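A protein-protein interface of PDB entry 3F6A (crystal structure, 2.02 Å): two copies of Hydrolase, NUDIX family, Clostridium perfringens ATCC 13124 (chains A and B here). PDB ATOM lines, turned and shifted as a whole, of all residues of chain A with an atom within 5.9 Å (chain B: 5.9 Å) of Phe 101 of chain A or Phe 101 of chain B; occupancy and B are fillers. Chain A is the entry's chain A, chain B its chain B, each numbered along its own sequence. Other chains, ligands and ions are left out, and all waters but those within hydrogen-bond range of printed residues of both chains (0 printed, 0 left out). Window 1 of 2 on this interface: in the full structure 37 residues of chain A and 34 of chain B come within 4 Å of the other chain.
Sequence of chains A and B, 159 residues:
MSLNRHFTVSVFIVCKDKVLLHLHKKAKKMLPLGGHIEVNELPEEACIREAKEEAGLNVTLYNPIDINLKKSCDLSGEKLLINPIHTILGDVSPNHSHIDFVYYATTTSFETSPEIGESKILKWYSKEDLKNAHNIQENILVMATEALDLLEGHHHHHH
Phe 7 of chain B touches its own counterpart, Phe 7 of chain A.
Pro 43 of chain A touches Ile 99 of chain B, and with the chains exchanged Ile 99 of chain A touches Pro 43 of chain B.
Pro 84 of chain A touches Thr 87 of chain B, and with the chains exchanged Thr 87 of chain A touches Pro 84 of chain B.
Phe 101 of chain B touches its own counterpart, Phe 101 of chain A.
The backbone carbonyl oxygen (O) of Pro 84 of chain A lies close to the side-chain amide oxygen (OD1) of Asn 83 of chain B (2.9 Å).
The side-chain amide nitrogen of Asn 83 of chain B lies within hydrogen-bond range of the side-chain hydroxyl of Thr 87 of chain A, at 2.6 Å.
Among the printed residues, merely in contact across the chains: His 86 of chain A with Asn 83 of chain B, Ile 99 of chain A with Pro 43 of chain B, Thr 87 of chain A with Pro 84 of chain B, Pro 43 of chain A with Ile 99 of chain B, Phe 7 of chain A with Phe 7 of chain B, Phe 101 of chain A with Phe 101 of chain B and Pro 84 of chain A with Thr 87 of chain B.
Phe 101 of chain A touches just one residue of chain B: Phe 101.
Of the printed residues of chain A, Ile 99 of chain B touches Pro 43 (3.4 Å).
Printed residues of chain B within 4 Å of Pro 43 of chain A: Ile 99.
Asp 100 of chain A touches none of the printed residues of chain B.
Ile 37 of chain B touches none of the printed residues of chain A.
N of Thr 8 of chain B lies within hydrogen-bond range of O of Ile 99 of chain B (3.1 Å).
N of Phe 101 of chain B lies within hydrogen-bond range of O of Thr 8 of chain B, 2.9 Å away.
O of Pro 43 of chain B is in hydrogen-bond range of SG of Cys 47 of chain B (3.6 Å).
The backbone carbonyl oxygen of Thr 8 of chain A is in hydrogen-bond range of the backbone NH of Phe 101 of chain A (2.9 Å).
The backbone NH of Ser 10 of chain A lies within hydrogen-bond range of the backbone carbonyl oxygen of Phe 101 of chain A (2.9 Å).
The backbone NH (N) of Val 102 of chain A is in hydrogen-bond range of the backbone carbonyl oxygen (O) of His 86 of chain A (2.9 Å).
Of the 18 printed residues of chain B, 7 touch a printed residue of chain A.
Hydrophobic or aromatic side chains of chain B that line the printed part of chain A: Phe 7, Pro 43, Pro 84, Ile 99 and Phe 101.
Along chain B the printed residues that touch a printed residue of chain A span positions 7 to 101.
Among the printed residues, no Asp or Glu carboxylate lies within 4 Å of a Lys or Arg side-chain nitrogen of the other chain.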
ATOM      1  N   PHE A   7       6.615  24.363  -1.784  1.00  0.00           N
ATOM      2  CA  PHE A   7       6.069  23.681  -2.951  1.00  0.00           C
ATOM      3  C   PHE A   7       4.823  22.879  -2.618  1.00  0.00           C
ATOM      4  O   PHE A   7       4.813  22.086  -1.673  1.00  0.00           O
ATOM      5  CB  PHE A   7       7.140  22.764  -3.548  1.00  0.00           C
ATOM      6  CG  PHE A   7       8.323  23.508  -4.109  1.00  0.00           C
ATOM      7  CD1 PHE A   7       8.364  23.867  -5.451  1.00  0.00           C
ATOM      8  CD2 PHE A   7       9.385  23.872  -3.287  1.00  0.00           C
ATOM      9  CE1 PHE A   7       9.446  24.588  -5.964  1.00  0.00           C
ATOM     10  CE2 PHE A   7      10.467  24.591  -3.790  1.00  0.00           C
ATOM     11  CZ  PHE A   7      10.500  24.946  -5.129  1.00  0.00           C
ATOM     12  N   THR A   8       3.776  23.092  -3.408  1.00  0.00           N
ATOM     13  CA  THR A   8       2.509  22.404  -3.223  1.00  0.00           C
ATOM     14  C   THR A   8       2.010  21.902  -4.577  1.00  0.00           C
ATOM     15  O   THR A   8       2.572  22.240  -5.620  1.00  0.00           O
ATOM     16  CB  THR A   8       1.439  23.361  -2.654  1.00  0.00           C
ATOM     17  OG1 THR A   8       1.081  24.326  -3.654  1.00  0.00           O
ATOM     18  CG2 THR A   8       1.967  24.101  -1.430  1.00  0.00           C
ATOM     19  N   VAL A   9       0.950  21.097  -4.556  1.00  0.00           N
ATOM     20  CA  VAL A   9       0.359  20.594  -5.788  1.00  0.00           C
ATOM     21  C   VAL A   9      -1.147  20.817  -5.755  1.00  0.00           C
ATOM     22  O   VAL A   9      -1.738  20.997  -4.689  1.00  0.00           O
ATOM     23  CB  VAL A   9       0.639  19.078  -6.006  1.00  0.00           C
ATOM     24  CG1 VAL A   9       2.133  18.833  -6.070  1.00  0.00           C
ATOM     25  CG2 VAL A   9      -0.010  18.240  -4.899  1.00  0.00           C
ATOM     26  N   SER A  10      -1.755  20.824  -6.935  1.00  0.00           N
ATOM     27  CA  SER A  10      -3.195  20.992  -7.083  1.00  0.00           C
ATOM     28  C   SER A  10      -3.607  19.989  -8.146  1.00  0.00           C
ATOM     29  O   SER A  10      -2.855  19.737  -9.084  1.00  0.00           O
ATOM     30  CB  SER A  10      -3.550  22.408  -7.561  1.00  0.00           C
ATOM     31  OG  SER A  10      -3.412  23.348  -6.514  1.00  0.00           O
ATOM     32  N   VAL A  11      -4.794  19.414  -7.996  1.00  0.00           N
ATOM     33  CA  VAL A  11      -5.278  18.438  -8.957  1.00  0.00           C
ATOM     34  C   VAL A  11      -6.739  18.668  -9.292  1.00  0.00           C
ATOM     35  O   VAL A  11      -7.588  18.697  -8.405  1.00  0.00           O
ATOM     36  CB  VAL A  11      -5.175  16.997  -8.419  1.00  0.00           C
ATOM     37  CG1 VAL A  11      -5.192  16.018  -9.579  1.00  0.00           C
ATOM     38  CG2 VAL A  11      -3.933  16.838  -7.579  1.00  0.00           C
ATOM     39  N   ILE A  37       3.882  18.944  -0.578  1.00  0.00           N
ATOM     40  CA  ILE A  37       4.580  17.786  -1.113  1.00  0.00           C
ATOM     41  C   ILE A  37       5.492  17.311   0.012  1.00  0.00           C
ATOM     42  O   ILE A  37       6.182  18.119   0.636  1.00  0.00           O
ATOM     43  CB  ILE A  37       5.459  18.177  -2.315  1.00  0.00           C
ATOM     44  CG1 ILE A  37       4.627  18.933  -3.355  1.00  0.00           C
ATOM     45  CG2 ILE A  37       6.080  16.931  -2.935  1.00  0.00           C
ATOM     46  CD1 ILE A  37       5.448  19.422  -4.547  1.00  0.00           C
ATOM     47  N   PRO A  43       6.213  15.382  -6.865  1.00  0.00           N
ATOM     48  CA  PRO A  43       4.987  16.182  -6.958  1.00  0.00           C
ATOM     49  C   PRO A  43       3.798  15.339  -7.431  1.00  0.00           C
ATOM     50  O   PRO A  43       2.671  15.552  -6.995  1.00  0.00           O
ATOM     51  CB  PRO A  43       5.360  17.270  -7.968  1.00  0.00           C
ATOM     52  CG  PRO A  43       6.839  17.477  -7.702  1.00  0.00           C
ATOM     53  CD  PRO A  43       7.336  16.047  -7.561  1.00  0.00           C
ATOM     54  N   CYS A  47       0.069  14.320  -5.655  1.00  0.00           N
ATOM     55  CA  CYS A  47      -1.262  14.483  -6.241  1.00  0.00           C
ATOM     56  C   CYS A  47      -2.074  13.229  -5.959  1.00  0.00           C
ATOM     57  O   CYS A  47      -3.233  13.302  -5.537  1.00  0.00           O
ATOM     58  CB  CYS A  47      -1.172  14.688  -7.754  1.00  0.00           C
ATOM     59  SG  CYS A  47      -0.537  16.301  -8.261  1.00  0.00           S
ATOM     60  N   PRO A  84       3.838  19.206 -14.698  1.00  0.00           N
ATOM     61  CA  PRO A  84       2.585  19.887 -14.351  1.00  0.00           C
ATOM     62  C   PRO A  84       2.018  20.576 -15.586  1.00  0.00           C
ATOM     63  O   PRO A  84       2.752  20.838 -16.534  1.00  0.00           O
ATOM     64  CB  PRO A  84       3.017  20.893 -13.283  1.00  0.00           C
ATOM     65  CG  PRO A  84       4.448  21.189 -13.644  1.00  0.00           C
ATOM     66  CD  PRO A  84       4.984  19.812 -13.996  1.00  0.00           C
ATOM     67  N   HIS A  86       0.341  23.514 -15.340  1.00  0.00           N
ATOM     68  CA  HIS A  86       0.619  24.917 -15.063  1.00  0.00           C
ATOM     69  C   HIS A  86       1.375  25.038 -13.751  1.00  0.00           C
ATOM     70  O   HIS A  86       1.345  24.128 -12.915  1.00  0.00           O
ATOM     71  CB  HIS A  86      -0.679  25.714 -14.935  1.00  0.00           C
ATOM     72  CG  HIS A  86      -1.478  25.797 -16.197  1.00  0.00           C
ATOM     73  ND1 HIS A  86      -0.977  26.340 -17.362  1.00  0.00           N
ATOM     74  CD2 HIS A  86      -2.757  25.446 -16.465  1.00  0.00           C
ATOM     75  CE1 HIS A  86      -1.914  26.319 -18.292  1.00  0.00           C
ATOM     76  NE2 HIS A  86      -3.005  25.783 -17.773  1.00  0.00           N
ATOM     77  N   THR A  87       2.041  26.175 -13.582  1.00  0.00           N
ATOM     78  CA  THR A  87       2.786  26.469 -12.370  1.00  0.00           C
ATOM     79  C   THR A  87       2.325  27.844 -11.898  1.00  0.00           C
ATOM     80  O   THR A  87       2.452  28.846 -12.615  1.00  0.00           O
ATOM     81  CB  THR A  87       4.306  26.479 -12.634  1.00  0.00           C
ATOM     82  OG1 THR A  87       4.727  25.170 -13.044  1.00  0.00           O
ATOM     83  CG2 THR A  87       5.061  26.872 -11.383  1.00  0.00           C
ATOM     84  N   ILE A  88       1.789  27.889 -10.683  1.00  0.00           N
ATOM     85  CA  ILE A  88       1.274  29.133 -10.121  1.00  0.00           C
ATOM     86  C   ILE A  88       1.874  29.515  -8.767  1.00  0.00           C
ATOM     87  O   ILE A  88       2.172  28.653  -7.933  1.00  0.00           O
ATOM     88  CB  ILE A  88      -0.260  29.039  -9.980  1.00  0.00           C
ATOM     89  CG1 ILE A  88      -0.883  28.839 -11.363  1.00  0.00           C
ATOM     90  CG2 ILE A  88      -0.812  30.289  -9.297  1.00  0.00           C
ATOM     91  CD1 ILE A  88      -2.383  28.604 -11.332  1.00  0.00           C
ATOM     92  N   ILE A  99       4.832  27.817  -4.421  1.00  0.00           N
ATOM     93  CA  ILE A  99       4.663  27.448  -5.811  1.00  0.00           C
ATOM     94  C   ILE A  99       3.656  26.311  -5.821  1.00  0.00           C
ATOM     95  O   ILE A  99       3.734  25.394  -5.003  1.00  0.00           O
ATOM     96  CB  ILE A  99       5.992  26.953  -6.416  1.00  0.00           C
ATOM     97  CG1 ILE A  99       6.938  28.137  -6.606  1.00  0.00           C
ATOM     98  CG2 ILE A  99       5.739  26.235  -7.736  1.00  0.00           C
ATOM     99  CD1 ILE A  99       8.314  27.745  -7.084  1.00  0.00           C
ATOM    100  N   ASP A 100       2.700  26.374  -6.736  1.00  0.00           N
ATOM    101  CA  ASP A 100       1.704  25.325  -6.832  1.00  0.00           C
ATOM    102  C   ASP A 100       1.740  24.684  -8.209  1.00  0.00           C
ATOM    103  O   ASP A 100       1.465  25.343  -9.220  1.00  0.00           O
ATOM    104  CB  ASP A 100       0.309  25.881  -6.556  1.00  0.00           C
ATOM    105  CG  ASP A 100      -0.765  24.816  -6.654  1.00  0.00           C
ATOM    106  OD1 ASP A 100      -0.752  23.872  -5.837  1.00  0.00           O
ATOM    107  OD2 ASP A 100      -1.619  24.919  -7.558  1.00  0.00           O
ATOM    108  N   PHE A 101       2.100  23.402  -8.241  1.00  0.00           N
ATOM    109  CA  PHE A 101       2.160  22.642  -9.484  1.00  0.00           C
ATOM    110  C   PHE A 101       0.783  22.067  -9.750  1.00  0.00           C
ATOM    111  O   PHE A 101       0.296  21.235  -8.990  1.00  0.00           O
ATOM    112  CB  PHE A 101       3.190  21.511  -9.378  1.00  0.00           C
ATOM    113  CG  PHE A 101       4.615  21.994  -9.350  1.00  0.00           C
ATOM    114  CD1 PHE A 101       5.067  22.914 -10.292  1.00  0.00           C
ATOM    115  CD2 PHE A 101       5.509  21.524  -8.394  1.00  0.00           C
ATOM    116  CE1 PHE A 101       6.389  23.358 -10.281  1.00  0.00           C
ATOM    117  CE2 PHE A 101       6.828  21.962  -8.376  1.00  0.00           C
ATOM    118  CZ  PHE A 101       7.268  22.879  -9.321  1.00  0.00           C
ATOM    119  N   VAL A 102       0.164  22.513 -10.840  1.00  0.00           N
ATOM    120  CA  VAL A 102      -1.181  22.081 -11.199  1.00  0.00           C
ATOM    121  C   VAL A 102      -1.242  20.920 -12.177  1.00  0.00           C
ATOM    122  O   VAL A 102      -0.633  20.963 -13.240  1.00  0.00           O
ATOM    123  CB  VAL A 102      -1.978  23.249 -11.793  1.00  0.00           C
ATOM    124  CG1 VAL A 102      -3.411  22.817 -12.069  1.00  0.00           C
ATOM    125  CG2 VAL A 102      -1.945  24.418 -10.840  1.00  0.00           C
ATOM    126  N   TYR A 103      -2.011  19.897 -11.813  1.00  0.00           N
ATOM    127  CA  TYR A 103      -2.179  18.708 -12.636  1.00  0.00           C
ATOM    128  C   TYR A 103      -3.652  18.463 -12.917  1.00  0.00           C
ATOM    129  O   TYR A 103      -4.517  18.851 -12.129  1.00  0.00           O
ATOM    130  CB  TYR A 103      -1.622  17.479 -11.908  1.00  0.00           C
ATOM    131  CG  TYR A 103      -0.133  17.499 -11.682  1.00  0.00           C
ATOM    132  CD1 TYR A 103       0.726  16.785 -12.514  1.00  0.00           C
ATOM    133  CD2 TYR A 103       0.424  18.232 -10.628  1.00  0.00           C
ATOM    134  CE1 TYR A 103       2.105  16.796 -12.307  1.00  0.00           C
ATOM    135  CE2 TYR A 103       1.802  18.247 -10.412  1.00  0.00           C
ATOM    136  CZ  TYR A 103       2.632  17.527 -11.258  1.00  0.00           C
ATOM    137  OH  TYR A 103       3.989  17.537 -11.057  1.00  0.00           O
ATOM    138  N   PHE B   7      16.359  20.968  -4.714  1.00  0.00           N
ATOM    139  CA  PHE B   7      15.841  20.998  -6.076  1.00  0.00           C
ATOM    140  C   PHE B   7      16.896  21.619  -6.972  1.00  0.00           C
ATOM    141  O   PHE B   7      17.698  22.431  -6.516  1.00  0.00           O
ATOM    142  CB  PHE B   7      14.585  21.864  -6.172  1.00  0.00           C
ATOM    143  CG  PHE B   7      13.326  21.168  -5.770  1.00  0.00           C
ATOM    144  CD1 PHE B   7      13.017  19.916  -6.281  1.00  0.00           C
ATOM    145  CD2 PHE B   7      12.412  21.795  -4.925  1.00  0.00           C
ATOM    146  CE1 PHE B   7      11.813  19.296  -5.960  1.00  0.00           C
ATOM    147  CE2 PHE B   7      11.207  21.184  -4.599  1.00  0.00           C
ATOM    148  CZ  PHE B   7      10.908  19.930  -5.120  1.00  0.00           C
ATOM    149  N   THR B   8      16.897  21.241  -8.245  1.00  0.00           N
ATOM    150  CA  THR B   8      17.841  21.812  -9.190  1.00  0.00           C
ATOM    151  C   THR B   8      17.096  22.225 -10.450  1.00  0.00           C
ATOM    152  O   THR B   8      15.934  21.860 -10.645  1.00  0.00           O
ATOM    153  CB  THR B   8      18.949  20.809  -9.577  1.00  0.00           C
ATOM    154  OG1 THR B   8      18.391  19.751 -10.365  1.00  0.00           O
ATOM    155  CG2 THR B   8      19.595  20.224  -8.328  1.00  0.00           C
ATOM    156  N   VAL B   9      17.761  23.008 -11.290  1.00  0.00           N
ATOM    157  CA  VAL B   9      17.188  23.445 -12.553  1.00  0.00           C
ATOM    158  C   VAL B   9      18.206  23.203 -13.663  1.00  0.00           C
ATOM    159  O   VAL B   9      19.410  23.101 -13.407  1.00  0.00           O
ATOM    160  CB  VAL B   9      16.830  24.957 -12.546  1.00  0.00           C
ATOM    161  CG1 VAL B   9      15.705  25.226 -11.567  1.00  0.00           C
ATOM    162  CG2 VAL B   9      18.050  25.780 -12.186  1.00  0.00           C
ATOM    163  N   SER B  10      17.704  23.100 -14.888  1.00  0.00           N
ATOM    164  CA  SER B  10      18.530  22.906 -16.067  1.00  0.00           C
ATOM    165  C   SER B  10      17.997  23.856 -17.122  1.00  0.00           C
ATOM    166  O   SER B  10      16.785  23.950 -17.304  1.00  0.00           O
ATOM    167  CB  SER B  10      18.406  21.468 -16.593  1.00  0.00           C
ATOM    168  OG  SER B  10      19.177  20.562 -15.829  1.00  0.00           O
ATOM    169  N   VAL B  11      18.881  24.578 -17.802  1.00  0.00           N
ATOM    170  CA  VAL B  11      18.420  25.470 -18.856  1.00  0.00           C
ATOM    171  C   VAL B  11      19.244  25.288 -20.127  1.00  0.00           C
ATOM    172  O   VAL B  11      20.476  25.335 -20.111  1.00  0.00           O
ATOM    173  CB  VAL B  11      18.434  26.968 -18.409  1.00  0.00           C
ATOM    174  CG1 VAL B  11      19.826  27.389 -17.979  1.00  0.00           C
ATOM    175  CG2 VAL B  11      17.950  27.844 -19.552  1.00  0.00           C
ATOM    176  N   ILE B  37      18.831  25.372  -6.473  1.00  0.00           N
ATOM    177  CA  ILE B  37      17.932  26.503  -6.314  1.00  0.00           C
ATOM    178  C   ILE B  37      18.140  27.072  -4.911  1.00  0.00           C
ATOM    179  O   ILE B  37      18.162  26.327  -3.928  1.00  0.00           O
ATOM    180  CB  ILE B  37      16.466  26.047  -6.501  1.00  0.00           C
ATOM    181  CG1 ILE B  37      16.326  25.345  -7.854  1.00  0.00           C
ATOM    182  CG2 ILE B  37      15.525  27.233  -6.422  1.00  0.00           C
ATOM    183  CD1 ILE B  37      14.920  24.847  -8.164  1.00  0.00           C
ATOM    184  N   PRO B  43      12.304  28.521  -9.320  1.00  0.00           N
ATOM    185  CA  PRO B  43      13.129  27.765 -10.265  1.00  0.00           C
ATOM    186  C   PRO B  43      13.484  28.606 -11.493  1.00  0.00           C
ATOM    187  O   PRO B  43      14.625  28.597 -11.945  1.00  0.00           O
ATOM    188  CB  PRO B  43      12.243  26.567 -10.611  1.00  0.00           C
ATOM    189  CG  PRO B  43      11.518  26.326  -9.330  1.00  0.00           C
ATOM    190  CD  PRO B  43      11.137  27.728  -8.890  1.00  0.00           C
ATOM    191  N   CYS B  47      17.217  29.756 -13.029  1.00  0.00           N
ATOM    192  CA  CYS B  47      17.688  29.607 -14.403  1.00  0.00           C
ATOM    193  C   CYS B  47      18.335  30.889 -14.923  1.00  0.00           C
ATOM    194  O   CYS B  47      19.410  30.861 -15.535  1.00  0.00           O
ATOM    195  CB  CYS B  47      16.529  29.242 -15.332  1.00  0.00           C
ATOM    196  SG  CYS B  47      15.930  27.545 -15.171  1.00  0.00           S
ATOM    197  N   ASN B  83       6.070  27.563 -16.820  1.00  0.00           N
ATOM    198  CA  ASN B  83       6.005  26.128 -16.547  1.00  0.00           C
ATOM    199  C   ASN B  83       7.294  25.436 -16.997  1.00  0.00           C
ATOM    200  O   ASN B  83       7.856  25.769 -18.042  1.00  0.00           O
ATOM    201  CB  ASN B  83       4.823  25.514 -17.306  1.00  0.00           C
ATOM    202  CG  ASN B  83       4.319  24.229 -16.674  1.00  0.00           C
ATOM    203  OD1 ASN B  83       4.139  23.221 -17.350  1.00  0.00           O
ATOM    204  ND2 ASN B  83       4.073  24.268 -15.375  1.00  0.00           N
ATOM    205  N   PRO B  84       7.785  24.465 -16.212  1.00  0.00           N
ATOM    206  CA  PRO B  84       9.012  23.790 -16.641  1.00  0.00           C
ATOM    207  C   PRO B  84       8.668  23.076 -17.945  1.00  0.00           C
ATOM    208  O   PRO B  84       7.501  22.779 -18.182  1.00  0.00           O
ATOM    209  CB  PRO B  84       9.283  22.794 -15.508  1.00  0.00           C
ATOM    210  CG  PRO B  84       8.591  23.414 -14.308  1.00  0.00           C
ATOM    211  CD  PRO B  84       7.313  23.950 -14.916  1.00  0.00           C
ATOM    212  N   HIS B  86      10.102  20.195 -18.757  1.00  0.00           N
ATOM    213  CA  HIS B  86      10.098  18.801 -18.314  1.00  0.00           C
ATOM    214  C   HIS B  86      10.498  18.751 -16.854  1.00  0.00           C
ATOM    215  O   HIS B  86      11.084  19.698 -16.337  1.00  0.00           O
ATOM    216  CB  HIS B  86      11.123  17.956 -19.086  1.00  0.00           C
ATOM    217  CG  HIS B  86      10.841  17.817 -20.549  1.00  0.00           C
ATOM    218  ND1 HIS B  86       9.677  17.266 -21.036  1.00  0.00           N
ATOM    219  CD2 HIS B  86      11.604  18.103 -21.630  1.00  0.00           C
ATOM    220  CE1 HIS B  86       9.733  17.216 -22.354  1.00  0.00           C
ATOM    221  NE2 HIS B  86      10.894  17.716 -22.740  1.00  0.00           N
ATOM    222  N   THR B  87      10.189  17.639 -16.198  1.00  0.00           N
ATOM    223  CA  THR B  87      10.571  17.451 -14.810  1.00  0.00           C
ATOM    224  C   THR B  87      11.266  16.099 -14.768  1.00  0.00           C
ATOM    225  O   THR B  87      10.692  15.085 -15.161  1.00  0.00           O
ATOM    226  CB  THR B  87       9.351  17.452 -13.878  1.00  0.00           C
ATOM    227  OG1 THR B  87       8.724  18.742 -13.918  1.00  0.00           O
ATOM    228  CG2 THR B  87       9.781  17.162 -12.449  1.00  0.00           C
ATOM    229  N   ILE B  88      12.505  16.083 -14.297  1.00  0.00           N
ATOM    230  CA  ILE B  88      13.266  14.843 -14.271  1.00  0.00           C
ATOM    231  C   ILE B  88      13.861  14.474 -12.921  1.00  0.00           C
ATOM    232  O   ILE B  88      14.299  15.336 -12.165  1.00  0.00           O
ATOM    233  CB  ILE B  88      14.411  14.917 -15.298  1.00  0.00           C
ATOM    234  CG1 ILE B  88      13.828  15.128 -16.697  1.00  0.00           C
ATOM    235  CG2 ILE B  88      15.270  13.653 -15.228  1.00  0.00           C
ATOM    236  CD1 ILE B  88      14.850  15.525 -17.743  1.00  0.00           C
ATOM    237  N   ILE B  99      15.092  16.104  -7.870  1.00  0.00           N
ATOM    238  CA  ILE B  99      14.214  16.583  -8.926  1.00  0.00           C
ATOM    239  C   ILE B  99      14.812  17.788  -9.633  1.00  0.00           C
ATOM    240  O   ILE B  99      15.224  18.758  -8.997  1.00  0.00           O
ATOM    241  CB  ILE B  99      12.830  16.968  -8.382  1.00  0.00           C
ATOM    242  CG1 ILE B  99      12.131  15.722  -7.845  1.00  0.00           C
ATOM    243  CG2 ILE B  99      11.990  17.601  -9.489  1.00  0.00           C
ATOM    244  CD1 ILE B  99      10.743  15.983  -7.273  1.00  0.00           C
ATOM    245  N   ASP B 100      14.848  17.715 -10.958  1.00  0.00           N
ATOM    246  CA  ASP B 100      15.398  18.778 -11.783  1.00  0.00           C
ATOM    247  C   ASP B 100      14.315  19.356 -12.684  1.00  0.00           C
ATOM    248  O   ASP B 100      13.627  18.616 -13.375  1.00  0.00           O
ATOM    249  CB  ASP B 100      16.541  18.228 -12.645  1.00  0.00           C
ATOM    250  CG  ASP B 100      17.225  19.308 -13.462  1.00  0.00           C
ATOM    251  OD1 ASP B 100      17.798  20.241 -12.858  1.00  0.00           O
ATOM    252  OD2 ASP B 100      17.189  19.232 -14.705  1.00  0.00           O
ATOM    253  N   PHE B 101      14.162  20.676 -12.657  1.00  0.00           N
ATOM    254  CA  PHE B 101      13.171  21.345 -13.489  1.00  0.00           C
ATOM    255  C   PHE B 101      13.891  21.867 -14.724  1.00  0.00           C
ATOM    256  O   PHE B 101      14.805  22.687 -14.613  1.00  0.00           O
ATOM    257  CB  PHE B 101      12.532  22.510 -12.729  1.00  0.00           C
ATOM    258  CG  PHE B 101      11.829  22.102 -11.469  1.00  0.00           C
ATOM    259  CD1 PHE B 101      10.683  21.313 -11.518  1.00  0.00           C
ATOM    260  CD2 PHE B 101      12.316  22.503 -10.226  1.00  0.00           C
ATOM    261  CE1 PHE B 101      10.028  20.929 -10.339  1.00  0.00           C
ATOM    262  CE2 PHE B 101      11.670  22.124  -9.049  1.00  0.00           C
ATOM    263  CZ  PHE B 101      10.526  21.336  -9.108  1.00  0.00           C
ATOM    264  N   VAL B 102      13.473  21.396 -15.897  1.00  0.00           N
ATOM    265  CA  VAL B 102      14.102  21.792 -17.149  1.00  0.00           C
ATOM    266  C   VAL B 102      13.367  22.899 -17.897  1.00  0.00           C
ATOM    267  O   VAL B 102      12.157  22.835 -18.101  1.00  0.00           O
ATOM    268  CB  VAL B 102      14.245  20.582 -18.096  1.00  0.00           C
ATOM    269  CG1 VAL B 102      14.957  20.991 -19.367  1.00  0.00           C
ATOM    270  CG2 VAL B 102      15.009  19.474 -17.400  1.00  0.00           C
ATOM    271  N   TYR B 103      14.121  23.905 -18.319  1.00  0.00           N
ATOM    272  CA  TYR B 103      13.572  25.035 -19.064  1.00  0.00           C
ATOM    273  C   TYR B 103      14.423  25.250 -20.305  1.00  0.00           C
ATOM    274  O   TYR B 103      15.604  24.898 -20.323  1.00  0.00           O
ATOM    275  CB  TYR B 103      13.625  26.302 -18.206  1.00  0.00           C
ATOM    276  CG  TYR B 103      12.752  26.259 -16.976  1.00  0.00           C
ATOM    277  CD1 TYR B 103      11.476  26.818 -16.985  1.00  0.00           C
ATOM    278  CD2 TYR B 103      13.202  25.658 -15.798  1.00  0.00           C
ATOM    279  CE1 TYR B 103      10.666  26.780 -15.849  1.00  0.00           C
ATOM    280  CE2 TYR B 103      12.398  25.621 -14.659  1.00  0.00           C
ATOM    281  CZ  TYR B 103      11.138  26.185 -14.694  1.00  0.00           C
ATOM    282  OH  TYR B 103      10.349  26.167 -13.573  1.00  0.00           O
